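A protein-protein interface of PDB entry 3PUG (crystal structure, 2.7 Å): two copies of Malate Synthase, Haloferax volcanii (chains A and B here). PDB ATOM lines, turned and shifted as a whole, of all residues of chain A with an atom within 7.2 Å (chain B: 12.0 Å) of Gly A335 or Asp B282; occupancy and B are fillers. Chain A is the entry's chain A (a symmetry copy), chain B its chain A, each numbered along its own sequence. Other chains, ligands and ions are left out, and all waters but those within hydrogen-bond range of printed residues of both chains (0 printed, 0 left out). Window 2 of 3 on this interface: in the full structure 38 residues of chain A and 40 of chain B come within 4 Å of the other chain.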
ATOM      1  N   ASP A 234     -17.237 -16.479  -6.248  1.00  0.00           N
ATOM      2  CA  ASP A 234     -17.098 -17.235  -5.041  1.00  0.00           C
ATOM      3  C   ASP A 234     -18.459 -17.896  -4.769  1.00  0.00           C
ATOM      4  O   ASP A 234     -19.259 -17.432  -3.956  1.00  0.00           O
ATOM      5  CB  ASP A 234     -16.645 -16.269  -3.953  1.00  0.00           C
ATOM      6  CG  ASP A 234     -16.092 -16.980  -2.735  1.00  0.00           C
ATOM      7  OD1 ASP A 234     -15.680 -16.235  -1.814  1.00  0.00           O
ATOM      8  OD2 ASP A 234     -16.082 -18.243  -2.686  1.00  0.00           O
ATOM      9  N   ASP A 237     -19.855 -18.754  -1.284  1.00  0.00           N
ATOM     10  CA  ASP A 237     -20.087 -17.629  -0.382  1.00  0.00           C
ATOM     11  C   ASP A 237     -21.515 -17.103  -0.527  1.00  0.00           C
ATOM     12  O   ASP A 237     -21.731 -15.951  -0.879  1.00  0.00           O
ATOM     13  CB  ASP A 237     -19.037 -16.551  -0.678  1.00  0.00           C
ATOM     14  CG  ASP A 237     -19.161 -15.326   0.200  1.00  0.00           C
ATOM     15  OD1 ASP A 237     -19.713 -15.422   1.313  1.00  0.00           O
ATOM     16  OD2 ASP A 237     -18.669 -14.251  -0.222  1.00  0.00           O
ATOM     17  N   GLU A 331     -12.519 -25.332   7.453  1.00  0.00           N
ATOM     18  CA  GLU A 331     -13.270 -25.478   6.204  1.00  0.00           C
ATOM     19  C   GLU A 331     -14.617 -24.729   6.150  1.00  0.00           C
ATOM     20  O   GLU A 331     -15.300 -24.725   5.125  1.00  0.00           O
ATOM     21  CB  GLU A 331     -13.404 -26.964   5.846  1.00  0.00           C
ATOM     22  CG  GLU A 331     -12.397 -27.463   4.801  1.00  0.00           C
ATOM     23  CD  GLU A 331     -12.987 -27.594   3.388  1.00  0.00           C
ATOM     24  OE1 GLU A 331     -14.017 -26.950   3.073  1.00  0.00           O
ATOM     25  OE2 GLU A 331     -12.417 -28.353   2.569  1.00  0.00           O
ATOM     26  N   GLU A 332     -15.017 -24.137   7.274  1.00  0.00           N
ATOM     27  CA  GLU A 332     -15.887 -22.962   7.294  1.00  0.00           C
ATOM     28  C   GLU A 332     -14.841 -21.861   7.341  1.00  0.00           C
ATOM     29  O   GLU A 332     -15.093 -20.710   6.982  1.00  0.00           O
ATOM     30  CB  GLU A 332     -16.725 -22.907   8.575  1.00  0.00           C
ATOM     31  CG  GLU A 332     -17.932 -21.955   8.535  1.00  0.00           C
ATOM     32  CD  GLU A 332     -19.115 -22.505   7.733  1.00  0.00           C
ATOM     33  OE1 GLU A 332     -19.938 -21.711   7.226  1.00  0.00           O
ATOM     34  OE2 GLU A 332     -19.243 -23.741   7.593  1.00  0.00           O
ATOM     35  N   LEU A 333     -13.663 -22.271   7.806  1.00  0.00           N
ATOM     36  CA  LEU A 333     -12.474 -21.441   7.946  1.00  0.00           C
ATOM     37  C   LEU A 333     -12.072 -20.831   6.599  1.00  0.00           C
ATOM     38  O   LEU A 333     -11.683 -19.658   6.554  1.00  0.00           O
ATOM     39  CB  LEU A 333     -11.328 -22.272   8.551  1.00  0.00           C
ATOM     40  CG  LEU A 333     -10.282 -21.625   9.474  1.00  0.00           C
ATOM     41  CD1 LEU A 333     -10.875 -21.218  10.829  1.00  0.00           C
ATOM     42  CD2 LEU A 333      -8.995 -22.452   9.650  1.00  0.00           C
ATOM     43  N   LEU A 334     -12.186 -21.607   5.515  1.00  0.00           N
ATOM     44  CA  LEU A 334     -11.902 -21.113   4.158  1.00  0.00           C
ATOM     45  C   LEU A 334     -12.697 -19.872   3.701  1.00  0.00           C
ATOM     46  O   LEU A 334     -12.139 -18.960   3.083  1.00  0.00           O
ATOM     47  CB  LEU A 334     -11.971 -22.236   3.112  1.00  0.00           C
ATOM     48  CG  LEU A 334     -10.860 -23.294   3.077  1.00  0.00           C
ATOM     49  CD1 LEU A 334     -10.710 -23.893   1.666  1.00  0.00           C
ATOM     50  CD2 LEU A 334      -9.504 -22.823   3.649  1.00  0.00           C
ATOM     51  N   GLY A 335     -13.993 -19.839   3.999  1.00  0.00           N
ATOM     52  CA  GLY A 335     -14.806 -18.645   3.784  1.00  0.00           C
ATOM     53  C   GLY A 335     -14.493 -17.507   4.746  1.00  0.00           C
ATOM     54  O   GLY A 335     -15.193 -16.487   4.747  1.00  0.00           O
ATOM     55  N   LEU A 336     -13.444 -17.699   5.552  1.00  0.00           N
ATOM     56  CA  LEU A 336     -12.953 -16.729   6.537  1.00  0.00           C
ATOM     57  C   LEU A 336     -11.482 -16.362   6.286  1.00  0.00           C
ATOM     58  O   LEU A 336     -10.929 -15.444   6.908  1.00  0.00           O
ATOM     59  CB  LEU A 336     -13.183 -17.258   7.964  1.00  0.00           C
ATOM     60  CG  LEU A 336     -14.554 -16.990   8.622  1.00  0.00           C
ATOM     61  CD1 LEU A 336     -15.662 -17.935   8.124  1.00  0.00           C
ATOM     62  CD2 LEU A 336     -14.526 -16.967  10.169  1.00  0.00           C
ATOM     63  N   THR A 337     -10.861 -17.091   5.359  1.00  0.00           N
ATOM     64  CA  THR A 337      -9.497 -16.807   4.922  1.00  0.00           C
ATOM     65  C   THR A 337      -9.327 -16.384   3.461  1.00  0.00           C
ATOM     66  O   THR A 337      -9.779 -17.059   2.526  1.00  0.00           O
ATOM     67  CB  THR A 337      -8.503 -17.959   5.190  1.00  0.00           C
ATOM     68  OG1 THR A 337      -8.872 -19.139   4.458  1.00  0.00           O
ATOM     69  CG2 THR A 337      -8.444 -18.229   6.670  1.00  0.00           C
ATOM     70  N   SER A 338      -8.621 -15.268   3.290  1.00  0.00           N
ATOM     71  CA  SER A 338      -8.116 -14.819   1.990  1.00  0.00           C
ATOM     72  C   SER A 338      -6.587 -14.722   1.976  1.00  0.00           C
ATOM     73  O   SER A 338      -5.959 -14.220   2.906  1.00  0.00           O
ATOM     74  CB  SER A 338      -8.798 -13.510   1.568  1.00  0.00           C
ATOM     75  OG  SER A 338      -9.233 -12.787   2.709  1.00  0.00           O
ATOM     76  N   SER B 278       0.937 -13.778   2.596  1.00  0.00           N
ATOM     77  CA  SER B 278       0.294 -13.308   3.825  1.00  0.00           C
ATOM     78  C   SER B 278      -1.100 -13.904   3.880  1.00  0.00           C
ATOM     79  O   SER B 278      -1.696 -14.093   2.824  1.00  0.00           O
ATOM     80  CB  SER B 278       0.201 -11.777   3.878  1.00  0.00           C
ATOM     81  OG  SER B 278       1.249 -11.191   4.634  1.00  0.00           O
ATOM     82  N   TRP B 279      -1.593 -14.208   5.084  1.00  0.00           N
ATOM     83  CA  TRP B 279      -2.880 -14.901   5.298  1.00  0.00           C
ATOM     84  C   TRP B 279      -3.873 -14.053   6.093  1.00  0.00           C
ATOM     85  O   TRP B 279      -3.512 -13.527   7.154  1.00  0.00           O
ATOM     86  CB  TRP B 279      -2.678 -16.253   5.998  1.00  0.00           C
ATOM     87  CG  TRP B 279      -2.339 -17.363   5.035  1.00  0.00           C
ATOM     88  CD1 TRP B 279      -1.086 -17.713   4.595  1.00  0.00           C
ATOM     89  CD2 TRP B 279      -3.260 -18.248   4.366  1.00  0.00           C
ATOM     90  NE1 TRP B 279      -1.172 -18.761   3.707  1.00  0.00           N
ATOM     91  CE2 TRP B 279      -2.489 -19.111   3.549  1.00  0.00           C
ATOM     92  CE3 TRP B 279      -4.657 -18.395   4.379  1.00  0.00           C
ATOM     93  CZ2 TRP B 279      -3.069 -20.112   2.751  1.00  0.00           C
ATOM     94  CZ3 TRP B 279      -5.233 -19.380   3.586  1.00  0.00           C
ATOM     95  CH2 TRP B 279      -4.439 -20.229   2.784  1.00  0.00           C
ATOM     96  N   LEU B 280      -5.105 -13.915   5.605  1.00  0.00           N
ATOM     97  CA  LEU B 280      -6.038 -13.009   6.274  1.00  0.00           C
ATOM     98  C   LEU B 280      -7.249 -13.714   6.845  1.00  0.00           C
ATOM     99  O   LEU B 280      -7.715 -14.688   6.269  1.00  0.00           O
ATOM    100  CB  LEU B 280      -6.487 -11.845   5.379  1.00  0.00           C
ATOM    101  CG  LEU B 280      -5.453 -10.808   4.910  1.00  0.00           C
ATOM    102  CD1 LEU B 280      -6.170  -9.618   4.277  1.00  0.00           C
ATOM    103  CD2 LEU B 280      -4.484 -10.359   6.023  1.00  0.00           C
ATOM    104  N   LEU B 281      -7.752 -13.182   7.958  1.00  0.00           N
ATOM    105  CA  LEU B 281      -8.800 -13.798   8.765  1.00  0.00           C
ATOM    106  C   LEU B 281     -10.000 -12.867   8.961  1.00  0.00           C
ATOM    107  O   LEU B 281      -9.802 -11.678   9.190  1.00  0.00           O
ATOM    108  CB  LEU B 281      -8.196 -14.107  10.139  1.00  0.00           C
ATOM    109  CG  LEU B 281      -8.801 -15.198  11.031  1.00  0.00           C
ATOM    110  CD1 LEU B 281      -8.342 -16.599  10.595  1.00  0.00           C
ATOM    111  CD2 LEU B 281      -8.462 -14.915  12.501  1.00  0.00           C
ATOM    112  N   ASP B 282     -11.226 -13.389   8.923  1.00  0.00           N
ATOM    113  CA  ASP B 282     -12.427 -12.599   9.236  1.00  0.00           C
ATOM    114  C   ASP B 282     -12.467 -11.930  10.626  1.00  0.00           C
ATOM    115  O   ASP B 282     -12.368 -12.565  11.683  1.00  0.00           O
ATOM    116  CB  ASP B 282     -13.693 -13.437   9.006  1.00  0.00           C
ATOM    117  CG  ASP B 282     -14.682 -12.771   8.043  1.00  0.00           C
ATOM    118  OD1 ASP B 282     -15.162 -11.654   8.347  1.00  0.00           O
ATOM    119  OD2 ASP B 282     -14.996 -13.359   6.981  1.00  0.00           O
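The backbone carbonyl oxygen (O) of Leu A336 sits close to the backbone carbonyl oxygen (O) of Leu B280. N of Leu B280 sits at hydrogen-bond distance from O of Ser A338, 2.8 Å away. O of Leu A336 sits at hydrogen-bond distance from N of Asp B282 (2.9 Å).
Among the printed residues, pairs that only touch across the chains: Gly A335 with Asp B282 (3.8 Å), Leu A336 with Leu B281 (3.3 Å), Thr A337 with Trp B279 (3.7 Å), Thr A337 with Leu B280 (3.1 Å) and Ser A338 with Trp B279 (3.8 Å).
Glu A331 touches none of the printed residues of chain B. No residue of chain B comes within 4 Å of Glu A332. Leu A333 touches none of the printed residues of chain B. No residue of chain B comes within 4 Å of Leu A334. Printed residues of chain B within 4 Å of Gly A335: Asp B282. Thr A337 touches two residues of chain B. Printed residues of chain B within 4 Å of Ser A338: Trp B279 and Leu B280. Printed residues of chain A within 4 Å of Trp B279: Thr A337 and Ser A338. Printed residues of chain A within 4 Å of Leu B280: Leu A336, Thr A337 and Ser A338. Of the printed residues of chain A, Leu B281 touches Leu A336 (3.3 Å). Printed residues of chain A within 4 Å of Asp B282: Gly A335 (3.8 Å) and Leu A336 (2.9 Å). The nearest residue of chain A that does not touch Asp B282 is Thr A337 (5.2 Å). The nearest printed residue of chain A that does not touch Leu B281 is Thr A337 (4.3 Å).
Hydrophobic or aromatic side chains of chain A that line the printed part of chain B: Leu A336.
No position is printed for both chains. Of the 8 pairs that touch across the chains among the printed residues, none has its exchanged pair printed and touching as well.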
